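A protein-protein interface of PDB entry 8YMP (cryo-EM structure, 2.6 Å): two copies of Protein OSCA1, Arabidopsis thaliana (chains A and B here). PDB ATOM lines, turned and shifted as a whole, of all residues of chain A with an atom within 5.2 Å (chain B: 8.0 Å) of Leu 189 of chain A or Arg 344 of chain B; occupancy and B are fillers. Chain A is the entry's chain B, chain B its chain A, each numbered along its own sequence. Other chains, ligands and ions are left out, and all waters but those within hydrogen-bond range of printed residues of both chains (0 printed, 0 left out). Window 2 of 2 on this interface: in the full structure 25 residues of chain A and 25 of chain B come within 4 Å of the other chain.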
ATOM      1  N   VAL A 184       5.701  19.549   4.949  1.00  0.00           N
ATOM      2  CA  VAL A 184       6.805  19.233   5.845  1.00  0.00           C
ATOM      3  C   VAL A 184       8.157  19.511   5.194  1.00  0.00           C
ATOM      4  O   VAL A 184       9.036  20.082   5.828  1.00  0.00           O
ATOM      5  CB  VAL A 184       6.723  17.790   6.374  1.00  0.00           C
ATOM      6  CG1 VAL A 184       7.908  17.478   7.270  1.00  0.00           C
ATOM      7  CG2 VAL A 184       5.430  17.599   7.146  1.00  0.00           C
ATOM      8  N   ALA A 185       8.331  19.143   3.929  1.00  0.00           N
ATOM      9  CA  ALA A 185       9.576  19.459   3.237  1.00  0.00           C
ATOM     10  C   ALA A 185       9.786  20.955   3.166  1.00  0.00           C
ATOM     11  O   ALA A 185      10.897  21.435   3.356  1.00  0.00           O
ATOM     12  CB  ALA A 185       9.589  18.867   1.845  1.00  0.00           C
ATOM     13  N   ASN A 186       8.725  21.701   2.898  1.00  0.00           N
ATOM     14  CA  ASN A 186       8.853  23.136   2.772  1.00  0.00           C
ATOM     15  C   ASN A 186       9.180  23.726   4.116  1.00  0.00           C
ATOM     16  O   ASN A 186       9.995  24.633   4.218  1.00  0.00           O
ATOM     17  CB  ASN A 186       7.566  23.745   2.244  1.00  0.00           C
ATOM     18  CG  ASN A 186       7.296  23.377   0.802  1.00  0.00           C
ATOM     19  OD1 ASN A 186       8.151  22.813   0.121  1.00  0.00           O
ATOM     20  ND2 ASN A 186       6.096  23.691   0.328  1.00  0.00           N
ATOM     21  N   MET A 187       8.553  23.209   5.158  1.00  0.00           N
ATOM     22  CA  MET A 187       8.794  23.715   6.491  1.00  0.00           C
ATOM     23  C   MET A 187      10.231  23.469   6.867  1.00  0.00           C
ATOM     24  O   MET A 187      10.881  24.345   7.407  1.00  0.00           O
ATOM     25  CB  MET A 187       7.886  23.016   7.484  1.00  0.00           C
ATOM     26  CG  MET A 187       6.576  23.725   7.769  1.00  0.00           C
ATOM     27  SD  MET A 187       5.512  22.726   8.827  1.00  0.00           S
ATOM     28  CE  MET A 187       3.904  23.107   8.143  1.00  0.00           C
ATOM     29  N   ARG A 188      10.735  22.279   6.576  1.00  0.00           N
ATOM     30  CA  ARG A 188      12.109  21.939   6.906  1.00  0.00           C
ATOM     31  C   ARG A 188      13.078  22.900   6.262  1.00  0.00           C
ATOM     32  O   ARG A 188      13.962  23.422   6.928  1.00  0.00           O
ATOM     33  CB  ARG A 188      12.423  20.503   6.490  1.00  0.00           C
ATOM     34  CG  ARG A 188      13.864  20.245   6.092  1.00  0.00           C
ATOM     35  CD  ARG A 188      14.444  19.080   6.865  1.00  0.00           C
ATOM     36  NE  ARG A 188      15.784  18.731   6.413  1.00  0.00           N
ATOM     37  CZ  ARG A 188      16.676  18.086   7.154  1.00  0.00           C
ATOM     38  NH1 ARG A 188      16.369  17.719   8.388  1.00  0.00           N
ATOM     39  NH2 ARG A 188      17.873  17.809   6.662  1.00  0.00           N
ATOM     40  N   LEU A 189      12.908  23.162   4.974  1.00  0.00           N
ATOM     41  CA  LEU A 189      13.833  24.032   4.263  1.00  0.00           C
ATOM     42  C   LEU A 189      13.719  25.480   4.719  1.00  0.00           C
ATOM     43  O   LEU A 189      14.723  26.183   4.788  1.00  0.00           O
ATOM     44  CB  LEU A 189      13.644  23.893   2.757  1.00  0.00           C
ATOM     45  CG  LEU A 189      14.084  22.543   2.200  1.00  0.00           C
ATOM     46  CD1 LEU A 189      13.864  22.494   0.700  1.00  0.00           C
ATOM     47  CD2 LEU A 189      15.541  22.282   2.542  1.00  0.00           C
ATOM     48  N   GLN A 190      12.517  25.929   5.057  1.00  0.00           N
ATOM     49  CA  GLN A 190      12.353  27.280   5.583  1.00  0.00           C
ATOM     50  C   GLN A 190      12.976  27.397   6.969  1.00  0.00           C
ATOM     51  O   GLN A 190      13.671  28.366   7.259  1.00  0.00           O
ATOM     52  CB  GLN A 190      10.875  27.649   5.634  1.00  0.00           C
ATOM     53  CG  GLN A 190      10.521  28.760   6.611  1.00  0.00           C
ATOM     54  CD  GLN A 190       9.359  28.395   7.516  1.00  0.00           C
ATOM     55  OE1 GLN A 190       8.277  28.971   7.414  1.00  0.00           O
ATOM     56  NE2 GLN A 190       9.579  27.432   8.407  1.00  0.00           N
ATOM     57  N   PHE A 191      12.750  26.407   7.821  1.00  0.00           N
ATOM     58  CA  PHE A 191      13.309  26.420   9.161  1.00  0.00           C
ATOM     59  C   PHE A 191      14.804  26.379   9.081  1.00  0.00           C
ATOM     60  O   PHE A 191      15.482  27.115   9.781  1.00  0.00           O
ATOM     61  CB  PHE A 191      12.820  25.204   9.935  1.00  0.00           C
ATOM     62  CG  PHE A 191      13.441  25.042  11.289  1.00  0.00           C
ATOM     63  CD1 PHE A 191      13.076  25.867  12.335  1.00  0.00           C
ATOM     64  CD2 PHE A 191      14.371  24.045  11.521  1.00  0.00           C
ATOM     65  CE1 PHE A 191      13.639  25.713  13.586  1.00  0.00           C
ATOM     66  CE2 PHE A 191      14.939  23.885  12.767  1.00  0.00           C
ATOM     67  CZ  PHE A 191      14.572  24.720  13.801  1.00  0.00           C
ATOM     68  N   LEU A 192      15.328  25.512   8.228  1.00  0.00           N
ATOM     69  CA  LEU A 192      16.766  25.372   8.112  1.00  0.00           C
ATOM     70  C   LEU A 192      17.379  26.718   7.811  1.00  0.00           C
ATOM     71  O   LEU A 192      18.405  27.073   8.380  1.00  0.00           O
ATOM     72  CB  LEU A 192      17.120  24.374   7.018  1.00  0.00           C
ATOM     73  CG  LEU A 192      17.719  23.032   7.434  1.00  0.00           C
ATOM     74  CD1 LEU A 192      17.033  22.496   8.676  1.00  0.00           C
ATOM     75  CD2 LEU A 192      17.614  22.037   6.290  1.00  0.00           C
ATOM     76  N   ALA A 193      16.749  27.476   6.923  1.00  0.00           N
ATOM     77  CA  ALA A 193      17.260  28.786   6.561  1.00  0.00           C
ATOM     78  C   ALA A 193      17.171  29.743   7.724  1.00  0.00           C
ATOM     79  O   ALA A 193      18.177  30.308   8.137  1.00  0.00           O
ATOM     80  CB  ALA A 193      16.500  29.331   5.377  1.00  0.00           C
ATOM     81  N   ALA A 680      14.874  16.782   0.409  1.00  0.00           N
ATOM     82  CA  ALA A 680      14.882  17.914   1.329  1.00  0.00           C
ATOM     83  C   ALA A 680      15.239  17.502   2.740  1.00  0.00           C
ATOM     84  O   ALA A 680      15.521  18.347   3.577  1.00  0.00           O
ATOM     85  CB  ALA A 680      13.534  18.597   1.323  1.00  0.00           C
ATOM     86  N   PRO A 685      20.912  21.325   0.257  1.00  0.00           N
ATOM     87  CA  PRO A 685      21.165  22.075  -0.966  1.00  0.00           C
ATOM     88  C   PRO A 685      22.369  22.980  -0.810  1.00  0.00           C
ATOM     89  O   PRO A 685      22.409  23.778   0.116  1.00  0.00           O
ATOM     90  CB  PRO A 685      19.900  22.908  -1.114  1.00  0.00           C
ATOM     91  CG  PRO A 685      18.839  22.090  -0.473  1.00  0.00           C
ATOM     92  CD  PRO A 685      19.510  21.439   0.695  1.00  0.00           C
ATOM     93  N   GLN A 687      23.091  25.458  -2.551  1.00  0.00           N
ATOM     94  CA  GLN A 687      22.635  26.827  -2.723  1.00  0.00           C
ATOM     95  C   GLN A 687      22.140  27.397  -1.423  1.00  0.00           C
ATOM     96  O   GLN A 687      22.447  28.533  -1.087  1.00  0.00           O
ATOM     97  CB  GLN A 687      21.506  26.879  -3.737  1.00  0.00           C
ATOM     98  CG  GLN A 687      21.067  28.285  -4.107  1.00  0.00           C
ATOM     99  CD  GLN A 687      19.562  28.422  -4.185  1.00  0.00           C
ATOM    100  OE1 GLN A 687      19.039  29.181  -4.999  1.00  0.00           O
ATOM    101  NE2 GLN A 687      18.857  27.686  -3.338  1.00  0.00           N
ATOM    102  N   GLU A 688      21.372  26.615  -0.680  1.00  0.00           N
ATOM    103  CA  GLU A 688      20.847  27.077   0.592  1.00  0.00           C
ATOM    104  C   GLU A 688      21.973  27.351   1.562  1.00  0.00           C
ATOM    105  O   GLU A 688      21.912  28.295   2.337  1.00  0.00           O
ATOM    106  CB  GLU A 688      19.894  26.044   1.172  1.00  0.00           C
ATOM    107  CG  GLU A 688      18.503  26.573   1.462  1.00  0.00           C
ATOM    108  CD  GLU A 688      17.627  26.596   0.228  1.00  0.00           C
ATOM    109  OE1 GLU A 688      16.776  27.501   0.117  1.00  0.00           O
ATOM    110  OE2 GLU A 688      17.792  25.708  -0.632  1.00  0.00           O
ATOM    111  N   PHE B 224      23.941  31.694 -11.016  1.00  0.00           N
ATOM    112  CA  PHE B 224      23.858  30.597 -10.070  1.00  0.00           C
ATOM    113  C   PHE B 224      25.212  30.021  -9.727  1.00  0.00           C
ATOM    114  O   PHE B 224      25.515  29.841  -8.557  1.00  0.00           O
ATOM    115  CB  PHE B 224      22.939  29.493 -10.581  1.00  0.00           C
ATOM    116  CG  PHE B 224      22.678  28.399  -9.584  1.00  0.00           C
ATOM    117  CD1 PHE B 224      21.722  28.555  -8.602  1.00  0.00           C
ATOM    118  CD2 PHE B 224      23.378  27.208  -9.641  1.00  0.00           C
ATOM    119  CE1 PHE B 224      21.475  27.550  -7.689  1.00  0.00           C
ATOM    120  CE2 PHE B 224      23.139  26.200  -8.732  1.00  0.00           C
ATOM    121  CZ  PHE B 224      22.185  26.370  -7.755  1.00  0.00           C
ATOM    122  N   THR B 341      23.859  18.108  -4.130  1.00  0.00           N
ATOM    123  CA  THR B 341      22.572  18.666  -4.527  1.00  0.00           C
ATOM    124  C   THR B 341      22.705  20.169  -4.600  1.00  0.00           C
ATOM    125  O   THR B 341      23.242  20.785  -3.687  1.00  0.00           O
ATOM    126  CB  THR B 341      21.468  18.291  -3.536  1.00  0.00           C
ATOM    127  OG1 THR B 341      20.611  19.419  -3.325  1.00  0.00           O
ATOM    128  CG2 THR B 341      22.067  17.856  -2.213  1.00  0.00           C
ATOM    129  N   GLN B 342      22.212  20.779  -5.670  1.00  0.00           N
ATOM    130  CA  GLN B 342      22.419  22.208  -5.853  1.00  0.00           C
ATOM    131  C   GLN B 342      21.321  23.140  -5.365  1.00  0.00           C
ATOM    132  O   GLN B 342      21.619  24.244  -4.921  1.00  0.00           O
ATOM    133  CB  GLN B 342      22.740  22.502  -7.312  1.00  0.00           C
ATOM    134  CG  GLN B 342      23.848  21.640  -7.876  1.00  0.00           C
ATOM    135  CD  GLN B 342      25.202  22.015  -7.325  1.00  0.00           C
ATOM    136  OE1 GLN B 342      25.517  23.194  -7.179  1.00  0.00           O
ATOM    137  NE2 GLN B 342      26.014  21.014  -7.016  1.00  0.00           N
ATOM    138  N   THR B 343      20.063  22.730  -5.447  1.00  0.00           N
ATOM    139  CA  THR B 343      18.984  23.629  -5.056  1.00  0.00           C
ATOM    140  C   THR B 343      17.821  22.922  -4.371  1.00  0.00           C
ATOM    141  O   THR B 343      17.698  21.704  -4.463  1.00  0.00           O
ATOM    142  CB  THR B 343      18.500  24.466  -6.252  1.00  0.00           C
ATOM    143  OG1 THR B 343      17.731  25.579  -5.783  1.00  0.00           O
ATOM    144  CG2 THR B 343      17.656  23.633  -7.187  1.00  0.00           C
ATOM    145  N   ARG B 344      16.973  23.677  -3.676  1.00  0.00           N
ATOM    146  CA  ARG B 344      15.836  23.097  -2.956  1.00  0.00           C
ATOM    147  C   ARG B 344      14.942  22.250  -3.826  1.00  0.00           C
ATOM    148  O   ARG B 344      14.556  21.156  -3.430  1.00  0.00           O
ATOM    149  CB  ARG B 344      14.997  24.193  -2.309  1.00  0.00           C
ATOM    150  CG  ARG B 344      15.052  25.531  -3.021  1.00  0.00           C
ATOM    151  CD  ARG B 344      14.010  26.478  -2.456  1.00  0.00           C
ATOM    152  NE  ARG B 344      14.242  26.759  -1.043  1.00  0.00           N
ATOM    153  CZ  ARG B 344      13.306  26.683  -0.103  1.00  0.00           C
ATOM    154  NH1 ARG B 344      12.069  26.329  -0.423  1.00  0.00           N
ATOM    155  NH2 ARG B 344      13.607  26.959   1.157  1.00  0.00           N
ATOM    156  N   ASN B 345      14.591  22.753  -5.002  1.00  0.00           N
ATOM    157  CA  ASN B 345      13.765  21.996  -5.932  1.00  0.00           C
ATOM    158  C   ASN B 345      14.579  20.859  -6.524  1.00  0.00           C
ATOM    159  O   ASN B 345      15.563  21.091  -7.220  1.00  0.00           O
ATOM    160  CB  ASN B 345      13.242  22.912  -7.034  1.00  0.00           C
ATOM    161  CG  ASN B 345      11.943  22.419  -7.636  1.00  0.00           C
ATOM    162  OD1 ASN B 345      11.757  22.453  -8.850  1.00  0.00           O
ATOM    163  ND2 ASN B 345      11.036  21.958  -6.786  1.00  0.00           N
ATOM    164  N   PRO B 346      14.166  19.614  -6.267  1.00  0.00           N
ATOM    165  CA  PRO B 346      14.960  18.479  -6.736  1.00  0.00           C
ATOM    166  C   PRO B 346      14.831  18.249  -8.224  1.00  0.00           C
ATOM    167  O   PRO B 346      15.418  17.305  -8.740  1.00  0.00           O
ATOM    168  CB  PRO B 346      14.346  17.310  -5.986  1.00  0.00           C
ATOM    169  CG  PRO B 346      12.925  17.702  -5.785  1.00  0.00           C
ATOM    170  CD  PRO B 346      12.933  19.188  -5.583  1.00  0.00           C
ATOM    171  N   THR B 347      14.072  19.091  -8.908  1.00  0.00           N
ATOM    172  CA  THR B 347      13.875  18.939 -10.338  1.00  0.00           C
ATOM    173  C   THR B 347      14.785  19.878 -11.096  1.00  0.00           C
ATOM    174  O   THR B 347      15.330  19.514 -12.133  1.00  0.00           O
ATOM    175  CB  THR B 347      12.418  19.233 -10.727  1.00  0.00           C
ATOM    176  OG1 THR B 347      11.655  19.510  -9.548  1.00  0.00           O
ATOM    177  CG2 THR B 347      11.813  18.043 -11.446  1.00  0.00           C
ATOM    178  N   GLU B 348      14.969  21.084 -10.577  1.00  0.00           N
ATOM    179  CA  GLU B 348      15.769  22.071 -11.280  1.00  0.00           C
ATOM    180  C   GLU B 348      17.233  22.026 -10.905  1.00  0.00           C
ATOM    181  O   GLU B 348      17.586  21.431  -9.893  1.00  0.00           O
ATOM    182  CB  GLU B 348      15.199  23.460 -11.039  1.00  0.00           C
ATOM    183  CG  GLU B 348      13.877  23.701 -11.740  1.00  0.00           C
ATOM    184  CD  GLU B 348      13.076  24.807 -11.093  1.00  0.00           C
ATOM    185  OE1 GLU B 348      13.429  25.214  -9.968  1.00  0.00           O
ATOM    186  OE2 GLU B 348      12.096  25.273 -11.709  1.00  0.00           O
ATOM    187  N   TRP B 349      18.082  22.657 -11.709  1.00  0.00           N
ATOM    188  CA  TRP B 349      19.523  22.646 -11.473  1.00  0.00           C
ATOM    189  C   TRP B 349      20.032  21.262 -11.132  1.00  0.00           C
ATOM    190  O   TRP B 349      20.487  21.029 -10.020  1.00  0.00           O
ATOM    191  CB  TRP B 349      19.919  23.624 -10.372  1.00  0.00           C
ATOM    192  CG  TRP B 349      19.574  25.058 -10.613  1.00  0.00           C
ATOM    193  CD1 TRP B 349      18.667  25.801  -9.924  1.00  0.00           C
ATOM    194  CD2 TRP B 349      20.158  25.938 -11.582  1.00  0.00           C
ATOM    195  NE1 TRP B 349      18.638  27.083 -10.405  1.00  0.00           N
ATOM    196  CE2 TRP B 349      19.544  27.192 -11.427  1.00  0.00           C
ATOM    197  CE3 TRP B 349      21.134  25.788 -12.566  1.00  0.00           C
ATOM    198  CZ2 TRP B 349      19.867  28.283 -12.223  1.00  0.00           C
ATOM    199  CZ3 TRP B 349      21.456  26.869 -13.351  1.00  0.00           C
ATOM    200  CH2 TRP B 349      20.825  28.102 -13.179  1.00  0.00           C
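O of Gln 342 of chain B sits close to N of Gln 687 of chain A (3.0 Å).
The guanidinium group (NE) of Arg 344 of chain B lies within salt-bridge range of the side-chain carboxylate (OE1) of Glu 688 of chain A, at 2.9 Å.
OG1 of Thr 343 of chain B lies within hydrogen-bond range of NE2 of Gln 687 of chain A (3.4 Å).
Leu 189 of chain A touches Arg 344 of chain B.
CA of Pro 685 of chain A touches OG1 of Thr 341 of chain B, at 3.6 Å.
Thr 343 of chain B touches Pro 685 of chain A (C to CB, 3.9 Å).
N of Arg 344 of chain B touches CB of Pro 685 of chain A (3.97 Å).
Gln 687 of chain A touches Phe 224 of chain B.
Leu 189 of chain A touches one residue of chain B.
Printed residues of chain B within 4 Å of Gln 687 of chain A: Phe 224, Gln 342 and Thr 343.
Of the printed residues of chain A, Phe 224 of chain B touches Gln 687.
Of the printed residues of chain A, Thr 341 of chain B touches Pro 685 (3.6 Å).
Of chain A, only Leu 189, Pro 685 and Glu 688 come within 4 Å of Arg 344 of chain B.
The nearest residue of chain A that does not touch Arg 344 of chain B is Gln 190 of chain A (4.2 Å).
The nearest printed residue of chain A that does not touch Thr 341 of chain B is Gln 687 of chain A (4.8 Å).
Of the 14 printed residues of chain A, 4 touch a printed residue of chain B.
Printed residues of chain A that touch a printed residue of chain B: Leu 189, Pro 685, Gln 687 and Glu 688.
Hydrophobic or aromatic side chains of chain A within 4 Å of the printed part of chain B: Leu 189 and Pro 685.
Among the printed residues, 8 pairs touch across the chains.
No position is printed for both chains.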
